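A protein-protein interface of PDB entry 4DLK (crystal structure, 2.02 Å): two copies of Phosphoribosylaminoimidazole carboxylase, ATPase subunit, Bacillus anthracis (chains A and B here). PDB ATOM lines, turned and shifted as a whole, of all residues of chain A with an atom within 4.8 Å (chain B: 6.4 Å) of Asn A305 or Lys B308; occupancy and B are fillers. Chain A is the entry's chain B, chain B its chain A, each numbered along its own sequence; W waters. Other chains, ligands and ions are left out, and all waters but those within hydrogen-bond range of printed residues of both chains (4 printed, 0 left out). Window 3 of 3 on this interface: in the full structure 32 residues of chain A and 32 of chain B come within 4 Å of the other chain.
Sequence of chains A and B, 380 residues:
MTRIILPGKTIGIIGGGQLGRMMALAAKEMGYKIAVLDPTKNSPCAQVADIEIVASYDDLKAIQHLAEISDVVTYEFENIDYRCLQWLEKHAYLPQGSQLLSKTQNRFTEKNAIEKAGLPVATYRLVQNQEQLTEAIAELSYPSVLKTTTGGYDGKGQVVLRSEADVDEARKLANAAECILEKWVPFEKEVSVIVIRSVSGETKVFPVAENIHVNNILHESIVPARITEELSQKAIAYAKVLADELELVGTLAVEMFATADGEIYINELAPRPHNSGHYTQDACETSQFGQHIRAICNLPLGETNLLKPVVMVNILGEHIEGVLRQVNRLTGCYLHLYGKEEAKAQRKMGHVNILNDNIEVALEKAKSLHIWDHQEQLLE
The side-chain amide nitrogen of Asn A305 sits close to the side-chain amino group of Lys B308 (3.5 Å).
N of Glu A303 is in hydrogen-bond range of OH of Tyr B334 (3.0 Å).
NZ of Lys B308 lies within salt-bridge range of OE2 of Glu A285.
The side-chain hydroxyl (OH) of Tyr B334 is in hydrogen-bond range of the side-chain carboxylate (OE1) of Glu A285.
N of Leu B307 is in hydrogen-bond range of O of Ala B283, 2.6 Å away.
O of Ala B283 lies within hydrogen-bond range of N of Lys B308 (3.5 Å).
O of Ala A283 sits at hydrogen-bond distance from N of Leu A307, 2.6 Å away.
The side-chain carboxylate of Glu A285 is in hydrogen-bond range of the side-chain amide nitrogen of Asn A305.
Glu A285 touches Leu B355.
CD1 of Leu B307 touches CB of Leu A307 (3.8 Å).
Of the printed residues of chain A, Tyr B334 touches Glu A285 and Glu A303.
Printed residues of chain B within 4 Å of Leu A307: Leu B307 (3.8 Å).
The nearest residue of chain A that does not touch Lys B308 is Leu A307 (4.5 Å).
Printed residues of chain B that touch a printed residue of chain A: Leu B307, Lys B308, Tyr B334 and Leu B355.
Hydrophobic or aromatic side chains of chain B within 4 Å of the printed part of chain A: Leu B307, Tyr B334 and Leu B355.
Hydrophobic or aromatic side chains of chain A that line the printed part of chain B: Leu A307.
Leu A307 touches its own counterpart, Leu B307.
Positions printed for both chains: 283, 284, 305, 306 and 307.
Water W2 bridges OE1 of Glu A285 (2.5 Å) and O of Leu B355 (2.9 Å).
Water W1 lies within hydrogen-bond range of O of Glu A285 (2.8 Å) and O of Asp B282 (2.8 Å).
Water W3 bridges O of Leu A307 (2.8 Å) and O of Leu B307 (2.8 Å).
Water W4 lies within hydrogen-bond range of the backbone carbonyl oxygen of Glu A285 (2.8 Å) and the side-chain carboxylate of Asp B282 (2.9 Å).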
ATOM      1  N   ALA A 283       9.354 -20.538  16.946  1.00  0.00           N
ATOM      2  CA  ALA A 283      10.627 -21.079  16.450  1.00  0.00           C
ATOM      3  C   ALA A 283      11.838 -20.171  16.648  1.00  0.00           C
ATOM      4  O   ALA A 283      12.988 -20.623  16.543  1.00  0.00           O
ATOM      5  CB  ALA A 283      10.495 -21.457  14.987  1.00  0.00           C
ATOM      6  N   CYS A 284      11.585 -18.899  16.934  1.00  0.00           N
ATOM      7  CA  CYS A 284      12.662 -17.942  17.153  1.00  0.00           C
ATOM      8  C   CYS A 284      12.751 -17.494  18.596  1.00  0.00           C
ATOM      9  O   CYS A 284      11.785 -17.591  19.355  1.00  0.00           O
ATOM     10  CB  CYS A 284      12.497 -16.722  16.249  1.00  0.00           C
ATOM     11  SG  CYS A 284      12.747 -17.109  14.511  1.00  0.00           S
ATOM     12  N   GLU A 285      13.924 -16.981  18.952  1.00  0.00           N
ATOM     13  CA  GLU A 285      14.192 -16.479  20.289  1.00  0.00           C
ATOM     14  C   GLU A 285      13.269 -15.313  20.668  1.00  0.00           C
ATOM     15  O   GLU A 285      12.884 -15.168  21.828  1.00  0.00           O
ATOM     16  CB  GLU A 285      15.665 -16.081  20.384  1.00  0.00           C
ATOM     17  CG  GLU A 285      16.173 -15.897  21.801  1.00  0.00           C
ATOM     18  CD  GLU A 285      17.688 -15.814  21.876  1.00  0.00           C
ATOM     19  OE1 GLU A 285      18.188 -15.004  22.679  1.00  0.00           O
ATOM     20  OE2 GLU A 285      18.377 -16.553  21.132  1.00  0.00           O
ATOM     21  N   GLU A 303      17.022 -11.275  20.303  1.00  0.00           N
ATOM     22  CA  GLU A 303      17.743 -12.017  19.283  1.00  0.00           C
ATOM     23  C   GLU A 303      16.743 -12.670  18.342  1.00  0.00           C
ATOM     24  O   GLU A 303      15.605 -12.955  18.738  1.00  0.00           O
ATOM     25  CB  GLU A 303      18.675 -13.055  19.907  1.00  0.00           C
ATOM     26  CG  GLU A 303      19.671 -12.482  20.909  1.00  0.00           C
ATOM     27  CD  GLU A 303      20.535 -11.368  20.333  1.00  0.00           C
ATOM     28  OE1 GLU A 303      21.092 -11.539  19.229  1.00  0.00           O
ATOM     29  OE2 GLU A 303      20.675 -10.320  20.991  1.00  0.00           O
ATOM     30  N   THR A 304      17.174 -12.896  17.104  1.00  0.00           N
ATOM     31  CA  THR A 304      16.326 -13.486  16.075  1.00  0.00           C
ATOM     32  C   THR A 304      16.789 -14.887  15.662  1.00  0.00           C
ATOM     33  O   THR A 304      16.405 -15.381  14.602  1.00  0.00           O
ATOM     34  CB  THR A 304      16.270 -12.592  14.814  1.00  0.00           C
ATOM     35  OG1 THR A 304      17.595 -12.414  14.302  1.00  0.00           O
ATOM     36  CG2 THR A 304      15.653 -11.225  15.133  1.00  0.00           C
ATOM     37  N   ASN A 305      17.602 -15.532  16.497  1.00  0.00           N
ATOM     38  CA  ASN A 305      18.073 -16.892  16.207  1.00  0.00           C
ATOM     39  C   ASN A 305      16.913 -17.851  15.993  1.00  0.00           C
ATOM     40  O   ASN A 305      15.930 -17.823  16.746  1.00  0.00           O
ATOM     41  CB  ASN A 305      18.951 -17.432  17.344  1.00  0.00           C
ATOM     42  CG  ASN A 305      20.069 -16.482  17.724  1.00  0.00           C
ATOM     43  OD1 ASN A 305      21.006 -16.268  16.959  1.00  0.00           O
ATOM     44  ND2 ASN A 305      19.978 -15.917  18.915  1.00  0.00           N
ATOM     45  N   LEU A 306      17.030 -18.691  14.968  1.00  0.00           N
ATOM     46  CA  LEU A 306      16.090 -19.778  14.763  1.00  0.00           C
ATOM     47  C   LEU A 306      16.449 -20.923  15.703  1.00  0.00           C
ATOM     48  O   LEU A 306      17.521 -21.524  15.587  1.00  0.00           O
ATOM     49  CB  LEU A 306      16.120 -20.262  13.316  1.00  0.00           C
ATOM     50  CG  LEU A 306      15.101 -21.337  12.935  1.00  0.00           C
ATOM     51  CD1 LEU A 306      13.706 -20.752  12.747  1.00  0.00           C
ATOM     52  CD2 LEU A 306      15.564 -22.055  11.672  1.00  0.00           C
ATOM     53  N   LEU A 307      15.546 -21.234  16.623  1.00  0.00           N
ATOM     54  CA  LEU A 307      15.851 -22.203  17.670  1.00  0.00           C
ATOM     55  C   LEU A 307      15.490 -23.629  17.279  1.00  0.00           C
ATOM     56  O   LEU A 307      16.007 -24.578  17.861  1.00  0.00           O
ATOM     57  CB  LEU A 307      15.206 -21.786  18.999  1.00  0.00           C
ATOM     58  CG  LEU A 307      15.689 -20.446  19.569  1.00  0.00           C
ATOM     59  CD1 LEU A 307      14.914 -20.082  20.828  1.00  0.00           C
ATOM     60  CD2 LEU A 307      17.188 -20.450  19.848  1.00  0.00           C
ATOM     61  N   VAL B 223      18.980 -23.100  34.149  1.00  0.00           N
ATOM     62  CA  VAL B 223      18.688 -24.270  33.315  1.00  0.00           C
ATOM     63  C   VAL B 223      19.633 -24.352  32.105  1.00  0.00           C
ATOM     64  O   VAL B 223      19.698 -23.406  31.315  1.00  0.00           O
ATOM     65  CB  VAL B 223      17.222 -24.272  32.818  1.00  0.00           C
ATOM     66  CG1 VAL B 223      16.852 -25.639  32.263  1.00  0.00           C
ATOM     67  CG2 VAL B 223      16.265 -23.908  33.945  1.00  0.00           C
ATOM     68  N   PRO B 224      20.360 -25.481  31.945  1.00  0.00           N
ATOM     69  CA  PRO B 224      20.353 -26.702  32.766  1.00  0.00           C
ATOM     70  C   PRO B 224      20.924 -26.485  34.159  1.00  0.00           C
ATOM     71  O   PRO B 224      21.901 -25.753  34.319  1.00  0.00           O
ATOM     72  CB  PRO B 224      21.273 -27.668  31.990  1.00  0.00           C
ATOM     73  CG  PRO B 224      21.490 -27.039  30.642  1.00  0.00           C
ATOM     74  CD  PRO B 224      21.376 -25.564  30.880  1.00  0.00           C
ATOM     75  N   ASP B 282      10.506 -18.627  27.546  1.00  0.00           N
ATOM     76  CA  ASP B 282      11.446 -18.146  26.541  1.00  0.00           C
ATOM     77  C   ASP B 282      12.474 -19.183  26.083  1.00  0.00           C
ATOM     78  O   ASP B 282      13.095 -19.020  25.029  1.00  0.00           O
ATOM     79  CB  ASP B 282      12.148 -16.883  27.063  1.00  0.00           C
ATOM     80  CG  ASP B 282      11.184 -15.705  27.215  1.00  0.00           C
ATOM     81  OD1 ASP B 282      10.598 -15.292  26.193  1.00  0.00           O
ATOM     82  OD2 ASP B 282      11.003 -15.198  28.345  1.00  0.00           O
ATOM     83  N   ALA B 283      12.658 -20.246  26.859  1.00  0.00           N
ATOM     84  CA  ALA B 283      13.769 -21.173  26.602  1.00  0.00           C
ATOM     85  C   ALA B 283      13.358 -22.567  26.148  1.00  0.00           C
ATOM     86  O   ALA B 283      14.195 -23.334  25.654  1.00  0.00           O
ATOM     87  CB  ALA B 283      14.675 -21.261  27.818  1.00  0.00           C
ATOM     88  N   CYS B 284      12.080 -22.895  26.315  1.00  0.00           N
ATOM     89  CA  CYS B 284      11.577 -24.210  25.930  1.00  0.00           C
ATOM     90  C   CYS B 284      10.630 -24.123  24.758  1.00  0.00           C
ATOM     91  O   CYS B 284      10.044 -23.069  24.486  1.00  0.00           O
ATOM     92  CB  CYS B 284      10.872 -24.900  27.102  1.00  0.00           C
ATOM     93  SG  CYS B 284      12.001 -25.396  28.412  1.00  0.00           S
ATOM     94  N   ASN B 305      11.578 -29.537  25.109  1.00  0.00           N
ATOM     95  CA  ASN B 305      12.999 -29.364  24.829  1.00  0.00           C
ATOM     96  C   ASN B 305      13.521 -28.012  25.261  1.00  0.00           C
ATOM     97  O   ASN B 305      12.876 -26.987  25.030  1.00  0.00           O
ATOM     98  CB  ASN B 305      13.275 -29.569  23.340  1.00  0.00           C
ATOM     99  CG  ASN B 305      12.873 -30.945  22.871  1.00  0.00           C
ATOM    100  OD1 ASN B 305      13.383 -31.953  23.360  1.00  0.00           O
ATOM    101  ND2 ASN B 305      11.950 -30.999  21.931  1.00  0.00           N
ATOM    102  N   LEU B 306      14.685 -28.016  25.901  1.00  0.00           N
ATOM    103  CA  LEU B 306      15.382 -26.776  26.205  1.00  0.00           C
ATOM    104  C   LEU B 306      16.045 -26.295  24.924  1.00  0.00           C
ATOM    105  O   LEU B 306      16.926 -26.965  24.386  1.00  0.00           O
ATOM    106  CB  LEU B 306      16.426 -26.982  27.309  1.00  0.00           C
ATOM    107  CG  LEU B 306      17.203 -25.730  27.738  1.00  0.00           C
ATOM    108  CD1 LEU B 306      16.328 -24.775  28.531  1.00  0.00           C
ATOM    109  CD2 LEU B 306      18.442 -26.110  28.534  1.00  0.00           C
ATOM    110  N   LEU B 307      15.615 -25.137  24.434  1.00  0.00           N
ATOM    111  CA  LEU B 307      16.099 -24.622  23.150  1.00  0.00           C
ATOM    112  C   LEU B 307      17.336 -23.753  23.305  1.00  0.00           C
ATOM    113  O   LEU B 307      18.141 -23.644  22.382  1.00  0.00           O
ATOM    114  CB  LEU B 307      14.981 -23.875  22.400  1.00  0.00           C
ATOM    115  CG  LEU B 307      13.778 -24.719  21.959  1.00  0.00           C
ATOM    116  CD1 LEU B 307      12.831 -23.889  21.109  1.00  0.00           C
ATOM    117  CD2 LEU B 307      14.215 -25.958  21.188  1.00  0.00           C
ATOM    118  N   LYS B 308      17.484 -23.146  24.478  1.00  0.00           N
ATOM    119  CA  LYS B 308      18.658 -22.350  24.805  1.00  0.00           C
ATOM    120  C   LYS B 308      18.813 -22.314  26.324  1.00  0.00           C
ATOM    121  O   LYS B 308      17.808 -22.213  27.039  1.00  0.00           O
ATOM    122  CB  LYS B 308      18.516 -20.924  24.248  1.00  0.00           C
ATOM    123  CG  LYS B 308      19.830 -20.152  24.119  1.00  0.00           C
ATOM    124  CD  LYS B 308      19.642 -18.886  23.289  1.00  0.00           C
ATOM    125  CE  LYS B 308      20.920 -18.061  23.199  1.00  0.00           C
ATOM    126  NZ  LYS B 308      21.005 -17.326  21.909  1.00  0.00           N
ATOM    127  N   PRO B 309      20.062 -22.416  26.827  1.00  0.00           N
ATOM    128  CA  PRO B 309      20.280 -22.245  28.265  1.00  0.00           C
ATOM    129  C   PRO B 309      19.791 -20.876  28.752  1.00  0.00           C
ATOM    130  O   PRO B 309      19.804 -19.898  27.994  1.00  0.00           O
ATOM    131  CB  PRO B 309      21.800 -22.355  28.405  1.00  0.00           C
ATOM    132  CG  PRO B 309      22.216 -23.216  27.260  1.00  0.00           C
ATOM    133  CD  PRO B 309      21.293 -22.842  26.131  1.00  0.00           C
ATOM    134  N   VAL B 310      19.376 -20.819  30.014  1.00  0.00           N
ATOM    135  CA  VAL B 310      18.645 -19.663  30.537  1.00  0.00           C
ATOM    136  C   VAL B 310      18.860 -19.440  32.036  1.00  0.00           C
ATOM    137  O   VAL B 310      19.019 -20.387  32.810  1.00  0.00           O
ATOM    138  CB  VAL B 310      17.124 -19.794  30.238  1.00  0.00           C
ATOM    139  CG1 VAL B 310      16.581 -21.144  30.710  1.00  0.00           C
ATOM    140  CG2 VAL B 310      16.327 -18.643  30.852  1.00  0.00           C
ATOM    141  N   TYR B 334      14.841 -11.210  28.401  1.00  0.00           N
ATOM    142  CA  TYR B 334      13.433 -11.214  28.015  1.00  0.00           C
ATOM    143  C   TYR B 334      12.562 -10.931  29.232  1.00  0.00           C
ATOM    144  O   TYR B 334      12.405 -11.774  30.115  1.00  0.00           O
ATOM    145  CB  TYR B 334      13.088 -12.514  27.264  1.00  0.00           C
ATOM    146  CG  TYR B 334      13.982 -12.658  26.044  1.00  0.00           C
ATOM    147  CD1 TYR B 334      15.215 -13.309  26.129  1.00  0.00           C
ATOM    148  CD2 TYR B 334      13.632 -12.072  24.832  1.00  0.00           C
ATOM    149  CE1 TYR B 334      16.059 -13.407  25.026  1.00  0.00           C
ATOM    150  CE2 TYR B 334      14.465 -12.158  23.725  1.00  0.00           C
ATOM    151  CZ  TYR B 334      15.679 -12.822  23.824  1.00  0.00           C
ATOM    152  OH  TYR B 334      16.509 -12.897  22.721  1.00  0.00           O
ATOM    153  N   LEU B 355      18.728 -15.377  28.236  1.00  0.00           N
ATOM    154  CA  LEU B 355      19.109 -16.486  27.359  1.00  0.00           C
ATOM    155  C   LEU B 355      20.530 -16.297  26.863  1.00  0.00           C
ATOM    156  O   LEU B 355      20.909 -15.192  26.478  1.00  0.00           O
ATOM    157  CB  LEU B 355      18.156 -16.581  26.164  1.00  0.00           C
ATOM    158  CG  LEU B 355      16.868 -17.414  26.266  1.00  0.00           C
ATOM    159  CD1 LEU B 355      16.039 -17.079  27.498  1.00  0.00           C
ATOM    160  CD2 LEU B 355      16.042 -17.203  25.013  1.00  0.00           C
ATOM    161  N   ASN B 356      21.307 -17.377  26.883  1.00  0.00           N
ATOM    162  CA  ASN B 356      22.682 -17.381  26.386  1.00  0.00           C
ATOM    163  C   ASN B 356      23.159 -18.812  26.190  1.00  0.00           C
ATOM    164  O   ASN B 356      22.769 -19.696  26.949  1.00  0.00           O
ATOM    165  CB  ASN B 356      23.621 -16.645  27.350  1.00  0.00           C
ATOM    166  CG  ASN B 356      24.933 -16.254  26.695  1.00  0.00           C
ATOM    167  OD1 ASN B 356      25.796 -17.096  26.442  1.00  0.00           O
ATOM    168  ND2 ASN B 356      25.082 -14.970  26.407  1.00  0.00           N
ATOM    169  N   ASP B 357      23.999 -19.039  25.179  1.00  0.00           N
ATOM    170  CA  ASP B 357      24.600 -20.363  24.946  1.00  0.00           C
ATOM    171  C   ASP B 357      25.415 -20.855  26.146  1.00  0.00           C
ATOM    172  O   ASP B 357      25.651 -22.050  26.294  1.00  0.00           O
ATOM    173  CB  ASP B 357      25.493 -20.349  23.701  1.00  0.00           C
ATOM    174  CG  ASP B 357      24.705 -20.201  22.412  1.00  0.00           C
ATOM    175  OD1 ASP B 357      25.157 -19.441  21.532  1.00  0.00           O
ATOM    176  OD2 ASP B 357      23.636 -20.838  22.274  1.00  0.00           O
HETATM  177  O   HOH W   1      11.893 -17.462  22.986  1.00  0.00           O
HETATM  178  O   HOH W   2      20.210 -14.059  23.900  1.00  0.00           O
HETATM  179  O   HOH W   3      18.051 -24.771  19.795  1.00  0.00           O
HETATM  180  O   HOH W   4      10.684 -14.348  23.412  1.00  0.00           O
